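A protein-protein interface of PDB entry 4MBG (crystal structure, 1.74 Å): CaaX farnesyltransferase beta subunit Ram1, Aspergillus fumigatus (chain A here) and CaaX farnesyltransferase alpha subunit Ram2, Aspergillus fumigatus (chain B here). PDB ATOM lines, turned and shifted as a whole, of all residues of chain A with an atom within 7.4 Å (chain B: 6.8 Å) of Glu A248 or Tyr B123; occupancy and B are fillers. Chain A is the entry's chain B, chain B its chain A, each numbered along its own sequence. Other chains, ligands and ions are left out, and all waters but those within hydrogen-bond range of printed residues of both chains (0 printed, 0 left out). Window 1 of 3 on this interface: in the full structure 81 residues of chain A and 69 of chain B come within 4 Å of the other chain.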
ATOM      1  N   SER A 150      -5.656   7.655   2.016  1.00  0.00           N
ATOM      2  CA  SER A 150      -7.131   7.740   1.902  1.00  0.00           C
ATOM      3  C   SER A 150      -7.768   8.605   2.981  1.00  0.00           C
ATOM      4  O   SER A 150      -8.991   8.621   3.140  1.00  0.00           O
ATOM      5  CB  SER A 150      -7.784   6.350   1.968  1.00  0.00           C
ATOM      6  OG  SER A 150      -7.329   5.511   0.936  1.00  0.00           O
ATOM      7  N   TRP A 153     -10.678  10.749   1.948  1.00  0.00           N
ATOM      8  CA  TRP A 153     -11.883   9.938   1.718  1.00  0.00           C
ATOM      9  C   TRP A 153     -12.574   9.595   3.023  1.00  0.00           C
ATOM     10  O   TRP A 153     -13.813   9.613   3.107  1.00  0.00           O
ATOM     11  CB  TRP A 153     -11.530   8.622   1.033  1.00  0.00           C
ATOM     12  CG  TRP A 153     -11.387   8.688  -0.454  1.00  0.00           C
ATOM     13  CD1 TRP A 153     -10.295   8.304  -1.191  1.00  0.00           C
ATOM     14  CD2 TRP A 153     -12.397   9.070  -1.399  1.00  0.00           C
ATOM     15  NE1 TRP A 153     -10.555   8.448  -2.531  1.00  0.00           N
ATOM     16  CE2 TRP A 153     -11.836   8.927  -2.688  1.00  0.00           C
ATOM     17  CE3 TRP A 153     -13.715   9.534  -1.281  1.00  0.00           C
ATOM     18  CZ2 TRP A 153     -12.543   9.239  -3.848  1.00  0.00           C
ATOM     19  CZ3 TRP A 153     -14.427   9.835  -2.442  1.00  0.00           C
ATOM     20  CH2 TRP A 153     -13.834   9.693  -3.702  1.00  0.00           C
ATOM     21  N   HIS A 199      -3.775  14.844  -5.614  1.00  0.00           N
ATOM     22  CA  HIS A 199      -4.433  13.741  -6.309  1.00  0.00           C
ATOM     23  C   HIS A 199      -5.897  14.158  -6.519  1.00  0.00           C
ATOM     24  O   HIS A 199      -6.517  14.745  -5.615  1.00  0.00           O
ATOM     25  CB  HIS A 199      -4.329  12.482  -5.423  1.00  0.00           C
ATOM     26  CG  HIS A 199      -4.758  11.208  -6.091  1.00  0.00           C
ATOM     27  ND1 HIS A 199      -6.083  10.912  -6.358  1.00  0.00           N
ATOM     28  CD2 HIS A 199      -4.043  10.131  -6.505  1.00  0.00           C
ATOM     29  CE1 HIS A 199      -6.163   9.715  -6.915  1.00  0.00           C
ATOM     30  NE2 HIS A 199      -4.938   9.215  -7.010  1.00  0.00           N
ATOM     31  N   VAL A 200      -6.458  13.884  -7.689  1.00  0.00           N
ATOM     32  CA  VAL A 200      -7.822  14.358  -7.940  1.00  0.00           C
ATOM     33  C   VAL A 200      -8.854  13.741  -6.987  1.00  0.00           C
ATOM     34  O   VAL A 200      -9.848  14.385  -6.671  1.00  0.00           O
ATOM     35  CB  VAL A 200      -8.305  14.142  -9.404  1.00  0.00           C
ATOM     36  CG1 VAL A 200      -7.421  14.866 -10.342  1.00  0.00           C
ATOM     37  CG2 VAL A 200      -8.400  12.638  -9.780  1.00  0.00           C
ATOM     38  N   LEU A 234      -2.954  17.788 -15.575  1.00  0.00           N
ATOM     39  CA  LEU A 234      -3.453  16.406 -15.656  1.00  0.00           C
ATOM     40  C   LEU A 234      -4.192  16.140 -16.963  1.00  0.00           C
ATOM     41  O   LEU A 234      -4.459  14.991 -17.318  1.00  0.00           O
ATOM     42  CB  LEU A 234      -4.384  16.121 -14.475  1.00  0.00           C
ATOM     43  CG  LEU A 234      -3.769  16.444 -13.106  1.00  0.00           C
ATOM     44  CD1 LEU A 234      -4.801  16.111 -12.036  1.00  0.00           C
ATOM     45  CD2 LEU A 234      -2.479  15.667 -12.852  1.00  0.00           C
ATOM     46  N   GLN A 236      -4.899  15.267 -20.584  1.00  0.00           N
ATOM     47  CA  GLN A 236      -4.116  14.424 -21.499  1.00  0.00           C
ATOM     48  C   GLN A 236      -4.492  14.658 -22.954  1.00  0.00           C
ATOM     49  O   GLN A 236      -5.586  15.113 -23.245  1.00  0.00           O
ATOM     50  CB  GLN A 236      -4.325  12.938 -21.146  1.00  0.00           C
ATOM     51  CG  GLN A 236      -3.858  12.627 -19.730  1.00  0.00           C
ATOM     52  CD  GLN A 236      -2.400  12.959 -19.530  1.00  0.00           C
ATOM     53  OE1 GLN A 236      -1.538  12.467 -20.261  1.00  0.00           O
ATOM     54  NE2 GLN A 236      -2.108  13.785 -18.528  1.00  0.00           N
ATOM     55  N   PHE A 241      -8.027  12.635 -18.163  1.00  0.00           N
ATOM     56  CA  PHE A 241      -7.208  13.212 -17.087  1.00  0.00           C
ATOM     57  C   PHE A 241      -6.483  12.110 -16.349  1.00  0.00           C
ATOM     58  O   PHE A 241      -7.069  11.065 -16.053  1.00  0.00           O
ATOM     59  CB  PHE A 241      -8.099  13.924 -16.051  1.00  0.00           C
ATOM     60  CG  PHE A 241      -8.704  15.202 -16.547  1.00  0.00           C
ATOM     61  CD1 PHE A 241      -9.881  15.184 -17.299  1.00  0.00           C
ATOM     62  CD2 PHE A 241      -8.092  16.424 -16.265  1.00  0.00           C
ATOM     63  CE1 PHE A 241     -10.438  16.377 -17.770  1.00  0.00           C
ATOM     64  CE2 PHE A 241      -8.649  17.624 -16.734  1.00  0.00           C
ATOM     65  CZ  PHE A 241      -9.815  17.599 -17.491  1.00  0.00           C
ATOM     66  N   THR A 242      -5.218  12.337 -16.029  1.00  0.00           N
ATOM     67  CA  THR A 242      -4.566  11.503 -15.032  1.00  0.00           C
ATOM     68  C   THR A 242      -5.032  11.892 -13.639  1.00  0.00           C
ATOM     69  O   THR A 242      -5.565  13.000 -13.433  1.00  0.00           O
ATOM     70  CB  THR A 242      -3.013  11.585 -15.121  1.00  0.00           C
ATOM     71  OG1 THR A 242      -2.593  12.964 -15.187  1.00  0.00           O
ATOM     72  CG2 THR A 242      -2.506  10.845 -16.366  1.00  0.00           C
ATOM     73  N   VAL A 243      -4.846  10.996 -12.666  1.00  0.00           N
ATOM     74  CA  VAL A 243      -5.321  11.288 -11.310  1.00  0.00           C
ATOM     75  C   VAL A 243      -4.320  12.118 -10.503  1.00  0.00           C
ATOM     76  O   VAL A 243      -4.677  12.730  -9.494  1.00  0.00           O
ATOM     77  CB  VAL A 243      -5.659   9.981 -10.541  1.00  0.00           C
ATOM     78  CG1 VAL A 243      -6.827   9.259 -11.235  1.00  0.00           C
ATOM     79  CG2 VAL A 243      -4.413   9.069 -10.441  1.00  0.00           C
ATOM     80  N   CYS A 244      -3.065  12.120 -10.957  1.00  0.00           N
ATOM     81  CA  CYS A 244      -2.010  12.936 -10.359  1.00  0.00           C
ATOM     82  C   CYS A 244      -0.874  12.933 -11.381  1.00  0.00           C
ATOM     83  O   CYS A 244      -0.904  12.167 -12.358  1.00  0.00           O
ATOM     84  CB  CYS A 244      -1.563  12.349  -8.997  1.00  0.00           C
ATOM     85  SG  CYS A 244      -0.846  10.692  -9.094  1.00  0.00           S
ATOM     86  N   GLU A 245       0.105  13.803 -11.200  1.00  0.00           N
ATOM     87  CA  GLU A 245       1.207  13.856 -12.158  1.00  0.00           C
ATOM     88  C   GLU A 245       1.991  12.558 -12.096  1.00  0.00           C
ATOM     89  O   GLU A 245       2.493  12.197 -11.037  1.00  0.00           O
ATOM     90  CB  GLU A 245       2.122  15.056 -11.858  1.00  0.00           C
ATOM     91  CG  GLU A 245       1.362  16.388 -11.955  1.00  0.00           C
ATOM     92  CD  GLU A 245       2.254  17.583 -11.689  1.00  0.00           C
ATOM     93  OE1 GLU A 245       3.081  17.908 -12.561  1.00  0.00           O
ATOM     94  OE2 GLU A 245       2.130  18.191 -10.612  1.00  0.00           O
ATOM     95  N   GLY A 246       2.061  11.852 -13.221  1.00  0.00           N
ATOM     96  CA  GLY A 246       2.750  10.575 -13.287  1.00  0.00           C
ATOM     97  C   GLY A 246       1.861   9.403 -12.917  1.00  0.00           C
ATOM     98  O   GLY A 246       2.322   8.261 -12.898  1.00  0.00           O
ATOM     99  N   GLY A 247       0.598   9.687 -12.609  1.00  0.00           N
ATOM    100  CA  GLY A 247      -0.370   8.657 -12.211  1.00  0.00           C
ATOM    101  C   GLY A 247      -1.251   8.124 -13.343  1.00  0.00           C
ATOM    102  O   GLY A 247      -1.112   8.528 -14.523  1.00  0.00           O
ATOM    103  N   GLU A 248      -2.162   7.213 -12.995  1.00  0.00           N
ATOM    104  CA  GLU A 248      -2.991   6.567 -13.997  1.00  0.00           C
ATOM    105  C   GLU A 248      -4.030   7.521 -14.621  1.00  0.00           C
ATOM    106  O   GLU A 248      -4.504   8.458 -13.983  1.00  0.00           O
ATOM    107  CB  GLU A 248      -3.735   5.367 -13.387  1.00  0.00           C
ATOM    108  CG  GLU A 248      -4.637   5.741 -12.197  1.00  0.00           C
ATOM    109  CD  GLU A 248      -3.958   5.631 -10.812  1.00  0.00           C
ATOM    110  OE1 GLU A 248      -2.752   5.885 -10.684  1.00  0.00           O
ATOM    111  OE2 GLU A 248      -4.655   5.306  -9.827  1.00  0.00           O
ATOM    112  N   GLU A 249      -4.382   7.230 -15.862  1.00  0.00           N
ATOM    113  CA  GLU A 249      -5.485   7.902 -16.554  1.00  0.00           C
ATOM    114  C   GLU A 249      -6.696   6.978 -16.613  1.00  0.00           C
ATOM    115  O   GLU A 249      -6.672   5.922 -17.263  1.00  0.00           O
ATOM    116  CB  GLU A 249      -5.092   8.280 -17.980  1.00  0.00           C
ATOM    117  CG  GLU A 249      -6.250   8.995 -18.684  1.00  0.00           C
ATOM    118  CD  GLU A 249      -5.931   9.484 -20.073  1.00  0.00           C
ATOM    119  OE1 GLU A 249      -4.802   9.258 -20.605  1.00  0.00           O
ATOM    120  OE2 GLU A 249      -6.838  10.139 -20.633  1.00  0.00           O
ATOM    121  N   ASP A 250      -7.766   7.376 -15.938  1.00  0.00           N
ATOM    122  CA  ASP A 250      -8.998   6.577 -15.994  1.00  0.00           C
ATOM    123  C   ASP A 250     -10.186   7.490 -15.797  1.00  0.00           C
ATOM    124  O   ASP A 250     -10.011   8.680 -15.525  1.00  0.00           O
ATOM    125  CB  ASP A 250      -8.962   5.378 -15.005  1.00  0.00           C
ATOM    126  CG  ASP A 250      -8.906   5.784 -13.538  1.00  0.00           C
ATOM    127  OD1 ASP A 250      -9.519   6.801 -13.140  1.00  0.00           O
ATOM    128  OD2 ASP A 250      -8.253   5.044 -12.756  1.00  0.00           O
ATOM    129  N   VAL A 251     -11.384   6.952 -15.980  1.00  0.00           N
ATOM    130  CA  VAL A 251     -12.589   7.797 -15.986  1.00  0.00           C
ATOM    131  C   VAL A 251     -12.908   8.379 -14.600  1.00  0.00           C
ATOM    132  O   VAL A 251     -13.561   9.406 -14.492  1.00  0.00           O
ATOM    133  CB  VAL A 251     -13.836   7.080 -16.590  1.00  0.00           C
ATOM    134  CG1 VAL A 251     -13.511   6.565 -18.012  1.00  0.00           C
ATOM    135  CG2 VAL A 251     -14.308   6.003 -15.698  1.00  0.00           C
ATOM    136  N   ARG A 252     -12.467   7.705 -13.542  1.00  0.00           N
ATOM    137  CA  ARG A 252     -12.613   8.231 -12.200  1.00  0.00           C
ATOM    138  C   ARG A 252     -11.808   9.540 -12.130  1.00  0.00           C
ATOM    139  O   ARG A 252     -12.247  10.526 -11.531  1.00  0.00           O
ATOM    140  CB  ARG A 252     -12.099   7.203 -11.162  1.00  0.00           C
ATOM    141  CG  ARG A 252     -11.553   7.880  -9.913  1.00  0.00           C
ATOM    142  CD  ARG A 252     -10.554   7.062  -9.108  1.00  0.00           C
ATOM    143  NE  ARG A 252      -9.410   6.616  -9.896  1.00  0.00           N
ATOM    144  CZ  ARG A 252      -8.203   6.349  -9.407  1.00  0.00           C
ATOM    145  NH1 ARG A 252      -7.936   6.530  -8.126  1.00  0.00           N
ATOM    146  NH2 ARG A 252      -7.248   5.912 -10.216  1.00  0.00           N
ATOM    147  N   GLY A 253     -10.648   9.569 -12.791  1.00  0.00           N
ATOM    148  CA  GLY A 253      -9.841  10.788 -12.847  1.00  0.00           C
ATOM    149  C   GLY A 253     -10.584  11.952 -13.519  1.00  0.00           C
ATOM    150  O   GLY A 253     -10.611  13.080 -13.010  1.00  0.00           O
ATOM    151  N   TYR B  88       0.645   6.283  -2.828  1.00  0.00           N
ATOM    152  CA  TYR B  88       0.758   6.522  -4.282  1.00  0.00           C
ATOM    153  C   TYR B  88       1.940   7.441  -4.601  1.00  0.00           C
ATOM    154  O   TYR B  88       2.627   7.262  -5.606  1.00  0.00           O
ATOM    155  CB  TYR B  88      -0.559   7.077  -4.907  1.00  0.00           C
ATOM    156  CG  TYR B  88      -0.963   8.420  -4.329  1.00  0.00           C
ATOM    157  CD1 TYR B  88      -0.541   9.611  -4.910  1.00  0.00           C
ATOM    158  CD2 TYR B  88      -1.747   8.492  -3.184  1.00  0.00           C
ATOM    159  CE1 TYR B  88      -0.872  10.851  -4.344  1.00  0.00           C
ATOM    160  CE2 TYR B  88      -2.087   9.721  -2.622  1.00  0.00           C
ATOM    161  CZ  TYR B  88      -1.643  10.897  -3.207  1.00  0.00           C
ATOM    162  OH  TYR B  88      -1.974  12.112  -2.630  1.00  0.00           O
ATOM    163  N   ILE B  92       5.327   6.938  -7.515  1.00  0.00           N
ATOM    164  CA  ILE B  92       5.640   7.903  -8.563  1.00  0.00           C
ATOM    165  C   ILE B  92       7.062   8.471  -8.418  1.00  0.00           C
ATOM    166  O   ILE B  92       7.793   8.597  -9.399  1.00  0.00           O
ATOM    167  CB  ILE B  92       4.565   9.004  -8.607  1.00  0.00           C
ATOM    168  CG1 ILE B  92       3.242   8.319  -8.977  1.00  0.00           C
ATOM    169  CG2 ILE B  92       4.945  10.101  -9.614  1.00  0.00           C
ATOM    170  CD1 ILE B  92       2.109   9.186  -8.955  1.00  0.00           C
ATOM    171  N   HIS B 119       0.732  -8.545  -2.567  1.00  0.00           N
ATOM    172  CA  HIS B 119      -0.409  -7.623  -2.440  1.00  0.00           C
ATOM    173  C   HIS B 119      -1.299  -7.731  -3.668  1.00  0.00           C
ATOM    174  O   HIS B 119      -1.304  -6.854  -4.535  1.00  0.00           O
ATOM    175  CB  HIS B 119       0.087  -6.178  -2.282  1.00  0.00           C
ATOM    176  CG  HIS B 119       1.032  -5.981  -1.133  1.00  0.00           C
ATOM    177  ND1 HIS B 119       0.604  -5.862   0.171  1.00  0.00           N
ATOM    178  CD2 HIS B 119       2.382  -5.866  -1.096  1.00  0.00           C
ATOM    179  CE1 HIS B 119       1.647  -5.693   0.965  1.00  0.00           C
ATOM    180  NE2 HIS B 119       2.739  -5.692   0.222  1.00  0.00           N
ATOM    181  N   LEU B 120      -2.039  -8.829  -3.754  1.00  0.00           N
ATOM    182  CA  LEU B 120      -2.856  -9.092  -4.943  1.00  0.00           C
ATOM    183  C   LEU B 120      -3.820  -7.984  -5.332  1.00  0.00           C
ATOM    184  O   LEU B 120      -4.071  -7.777  -6.516  1.00  0.00           O
ATOM    185  CB  LEU B 120      -3.666 -10.362  -4.744  1.00  0.00           C
ATOM    186  CG  LEU B 120      -2.859 -11.636  -4.569  1.00  0.00           C
ATOM    187  CD1 LEU B 120      -3.868 -12.802  -4.463  1.00  0.00           C
ATOM    188  CD2 LEU B 120      -1.886 -11.836  -5.734  1.00  0.00           C
ATOM    189  N   LYS B 121      -4.393  -7.303  -4.345  1.00  0.00           N
ATOM    190  CA  LYS B 121      -5.444  -6.333  -4.624  1.00  0.00           C
ATOM    191  C   LYS B 121      -4.920  -4.919  -4.878  1.00  0.00           C
ATOM    192  O   LYS B 121      -5.689  -4.014  -5.160  1.00  0.00           O
ATOM    193  CB  LYS B 121      -6.514  -6.367  -3.496  1.00  0.00           C
ATOM    194  CG  LYS B 121      -7.201  -7.763  -3.411  1.00  0.00           C
ATOM    195  CD  LYS B 121      -8.193  -7.933  -2.282  1.00  0.00           C
ATOM    196  CE  LYS B 121      -8.534  -9.424  -2.117  1.00  0.00           C
ATOM    197  NZ  LYS B 121      -9.695  -9.724  -1.227  1.00  0.00           N
ATOM    198  N   ASN B 122      -3.601  -4.747  -4.829  1.00  0.00           N
ATOM    199  CA  ASN B 122      -2.999  -3.412  -4.965  1.00  0.00           C
ATOM    200  C   ASN B 122      -2.889  -3.001  -6.422  1.00  0.00           C
ATOM    201  O   ASN B 122      -2.264  -3.709  -7.215  1.00  0.00           O
ATOM    202  CB  ASN B 122      -1.608  -3.420  -4.320  1.00  0.00           C
ATOM    203  CG  ASN B 122      -0.919  -2.077  -4.381  1.00  0.00           C
ATOM    204  OD1 ASN B 122      -0.554  -1.591  -5.467  1.00  0.00           O
ATOM    205  ND2 ASN B 122      -0.710  -1.470  -3.216  1.00  0.00           N
ATOM    206  N   TYR B 123      -3.483  -1.864  -6.783  1.00  0.00           N
ATOM    207  CA  TYR B 123      -3.446  -1.436  -8.181  1.00  0.00           C
ATOM    208  C   TYR B 123      -2.297  -0.459  -8.524  1.00  0.00           C
ATOM    209  O   TYR B 123      -1.907  -0.341  -9.689  1.00  0.00           O
ATOM    210  CB  TYR B 123      -4.808  -0.874  -8.593  1.00  0.00           C
ATOM    211  CG  TYR B 123      -5.226   0.304  -7.765  1.00  0.00           C
ATOM    212  CD1 TYR B 123      -4.785   1.580  -8.085  1.00  0.00           C
ATOM    213  CD2 TYR B 123      -6.040   0.146  -6.640  1.00  0.00           C
ATOM    214  CE1 TYR B 123      -5.150   2.671  -7.334  1.00  0.00           C
ATOM    215  CE2 TYR B 123      -6.420   1.257  -5.870  1.00  0.00           C
ATOM    216  CZ  TYR B 123      -5.961   2.508  -6.227  1.00  0.00           C
ATOM    217  OH  TYR B 123      -6.311   3.621  -5.499  1.00  0.00           O
ATOM    218  N   GLN B 124      -1.750   0.214  -7.514  1.00  0.00           N
ATOM    219  CA  GLN B 124      -0.653   1.161  -7.712  1.00  0.00           C
ATOM    220  C   GLN B 124       0.554   0.453  -8.352  1.00  0.00           C
ATOM    221  O   GLN B 124       1.232   0.994  -9.232  1.00  0.00           O
ATOM    222  CB  GLN B 124      -0.246   1.787  -6.352  1.00  0.00           C
ATOM    223  CG  GLN B 124      -1.339   2.693  -5.706  1.00  0.00           C
ATOM    224  CD  GLN B 124      -2.286   1.966  -4.747  1.00  0.00           C
ATOM    225  OE1 GLN B 124      -2.447   0.744  -4.806  1.00  0.00           O
ATOM    226  NE2 GLN B 124      -2.944   2.736  -3.875  1.00  0.00           N
ATOM    227  N   ILE B 125       0.806  -0.764  -7.886  1.00  0.00           N
ATOM    228  CA  ILE B 125       1.854  -1.662  -8.400  1.00  0.00           C
ATOM    229  C   ILE B 125       1.730  -1.873  -9.911  1.00  0.00           C
ATOM    230  O   ILE B 125       2.734  -1.991 -10.632  1.00  0.00           O
ATOM    231  CB  ILE B 125       1.713  -3.027  -7.665  1.00  0.00           C
ATOM    232  CG1 ILE B 125       2.249  -2.916  -6.229  1.00  0.00           C
ATOM    233  CG2 ILE B 125       2.383  -4.198  -8.439  1.00  0.00           C
ATOM    234  CD1 ILE B 125       1.792  -4.081  -5.292  1.00  0.00           C
ATOM    235  N   TRP B 126       0.488  -1.908 -10.387  1.00  0.00           N
ATOM    236  CA  TRP B 126       0.210  -2.221 -11.796  1.00  0.00           C
ATOM    237  C   TRP B 126       0.303  -0.982 -12.683  1.00  0.00           C
ATOM    238  O   TRP B 126       0.698  -1.076 -13.841  1.00  0.00           O
ATOM    239  CB  TRP B 126      -1.099  -3.031 -11.964  1.00  0.00           C
ATOM    240  CG  TRP B 126      -0.832  -4.397 -11.385  1.00  0.00           C
ATOM    241  CD1 TRP B 126      -0.949  -4.771 -10.062  1.00  0.00           C
ATOM    242  CD2 TRP B 126      -0.261  -5.521 -12.067  1.00  0.00           C
ATOM    243  NE1 TRP B 126      -0.517  -6.072  -9.902  1.00  0.00           N
ATOM    244  CE2 TRP B 126      -0.073  -6.545 -11.110  1.00  0.00           C
ATOM    245  CE3 TRP B 126       0.136  -5.752 -13.394  1.00  0.00           C
ATOM    246  CZ2 TRP B 126       0.457  -7.801 -11.445  1.00  0.00           C
ATOM    247  CZ3 TRP B 126       0.674  -6.996 -13.725  1.00  0.00           C
ATOM    248  CH2 TRP B 126       0.833  -8.007 -12.756  1.00  0.00           C
ATOM    249  N   HIS B 127      -0.008   0.193 -12.136  1.00  0.00           N
ATOM    250  CA  HIS B 127       0.328   1.407 -12.876  1.00  0.00           C
ATOM    251  C   HIS B 127       1.853   1.557 -13.001  1.00  0.00           C
ATOM    252  O   HIS B 127       2.377   1.915 -14.061  1.00  0.00           O
ATOM    253  CB  HIS B 127      -0.240   2.663 -12.223  1.00  0.00           C
ATOM    254  CG  HIS B 127       0.145   3.914 -12.955  1.00  0.00           C
ATOM    255  ND1 HIS B 127      -0.289   4.181 -14.236  1.00  0.00           N
ATOM    256  CD2 HIS B 127       0.974   4.934 -12.615  1.00  0.00           C
ATOM    257  CE1 HIS B 127       0.246   5.319 -14.651  1.00  0.00           C
ATOM    258  NE2 HIS B 127       1.009   5.801 -13.684  1.00  0.00           N
ATOM    259  N   HIS B 128       2.559   1.296 -11.901  1.00  0.00           N
ATOM    260  CA  HIS B 128       4.030   1.381 -11.891  1.00  0.00           C
ATOM    261  C   HIS B 128       4.592   0.432 -12.958  1.00  0.00           C
ATOM    262  O   HIS B 128       5.500   0.793 -13.716  1.00  0.00           O
ATOM    263  CB  HIS B 128       4.548   1.012 -10.478  1.00  0.00           C
ATOM    264  CG  HIS B 128       6.022   1.218 -10.280  1.00  0.00           C
ATOM    265  ND1 HIS B 128       6.604   2.470 -10.245  1.00  0.00           N
ATOM    266  CD2 HIS B 128       7.027   0.329 -10.084  1.00  0.00           C
ATOM    267  CE1 HIS B 128       7.904   2.343 -10.035  1.00  0.00           C
ATOM    268  NE2 HIS B 128       8.186   1.056  -9.923  1.00  0.00           N
ATOM    269  N   GLN B 130       3.191  -0.514 -15.749  1.00  0.00           N
ATOM    270  CA  GLN B 130       2.928   0.060 -17.070  1.00  0.00           C
ATOM    271  C   GLN B 130       3.946   1.190 -17.373  1.00  0.00           C
ATOM    272  O   GLN B 130       4.455   1.312 -18.505  1.00  0.00           O
ATOM    273  CB  GLN B 130       1.496   0.598 -17.107  1.00  0.00           C
ATOM    274  CG  GLN B 130       1.127   1.304 -18.422  1.00  0.00           C
ATOM    275  CD  GLN B 130      -0.316   1.784 -18.446  1.00  0.00           C
ATOM    276  OE1 GLN B 130      -1.211   1.170 -17.853  1.00  0.00           O
ATOM    277  NE2 GLN B 130      -0.549   2.894 -19.143  1.00  0.00           N
ATOM    278  N   HIS B 162      -7.247  -4.757 -12.227  1.00  0.00           N
ATOM    279  CA  HIS B 162      -5.998  -4.028 -12.539  1.00  0.00           C
ATOM    280  C   HIS B 162      -5.013  -4.847 -13.402  1.00  0.00           C
ATOM    281  O   HIS B 162      -4.302  -4.285 -14.265  1.00  0.00           O
ATOM    282  CB  HIS B 162      -5.298  -3.499 -11.264  1.00  0.00           C
ATOM    283  CG  HIS B 162      -5.235  -4.475 -10.114  1.00  0.00           C
ATOM    284  ND1 HIS B 162      -6.323  -4.761  -9.314  1.00  0.00           N
ATOM    285  CD2 HIS B 162      -4.197  -5.186  -9.601  1.00  0.00           C
ATOM    286  CE1 HIS B 162      -5.960  -5.606  -8.360  1.00  0.00           C
ATOM    287  NE2 HIS B 162      -4.672  -5.881  -8.513  1.00  0.00           N
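A ring nitrogen (NE2) of His B127 is in hydrogen-bond range of the backbone carbonyl oxygen of Gly A246 (2.9 Å).
Hydrophobic or aromatic side chains of chain B that line the printed part of chain A: Tyr B88, Ile B92, Tyr B123 and His B127.
Along chain B the printed residues that touch a printed residue of chain A span positions 88 to 127.
Of the 19 printed residues of chain A, 6 touch a printed residue of chain B.
Hydrophobic or aromatic side chains of chain A within 4 Å of the printed part of chain B: His A199.
Among the printed residues, 9 pairs touch across the chains.
Among the printed residues, no Asp or Glu carboxylate lies within 4 Å of a Lys or Arg side-chain nitrogen of the other chain.
Of chain B, only Tyr B123 and His B127 come within 4 Å of Glu A248.
Of chain A, only Glu A248 (3.7 Å) comes within 4 Å of Tyr B123.
Of the printed residues of chain B, Cys A244 touches Ile B92 (3.3 Å).
Of the printed residues of chain B, His A199 touches Tyr B88 (3.7 Å).
Of the printed residues of chain A, Ile B92 touches Cys A244, Glu A245, Gly A246 and Gly A247.
Glu A249 touches none of the printed residues of chain B.
Gln A236 touches none of the printed residues of chain B.
The nearest residue of chain B that does not touch Glu A248 is Gln B124 (5.9 Å).
The nearest residue of chain A that does not touch Tyr B123 is Arg A252 (4.2 Å).
O of Cys A244 lies within hydrogen-bond range of OG1 of Thr A242, at 3.4 Å.
The side-chain carboxylate of Glu A248 is in salt-bridge range of the guanidinium group of Arg A252, at 2.7 Å.
N of Val A243 sits at hydrogen-bond distance from O of Glu A248.
Among the printed residues, pairs that only touch across the chains: His A199 with Tyr B88 (3.7 Å), Cys A244 with Ile B92 (3.3 Å), Glu A245 with Ile B92 (3.5 Å), Gly A246 with Ile B92 (3.98 Å), Gly A247 with Ile B92 (3.99 Å), Gly A247 with His B127 (3.3 Å), Glu A248 with Tyr B123 (3.7 Å) and Glu A248 with His B127 (3.5 Å).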
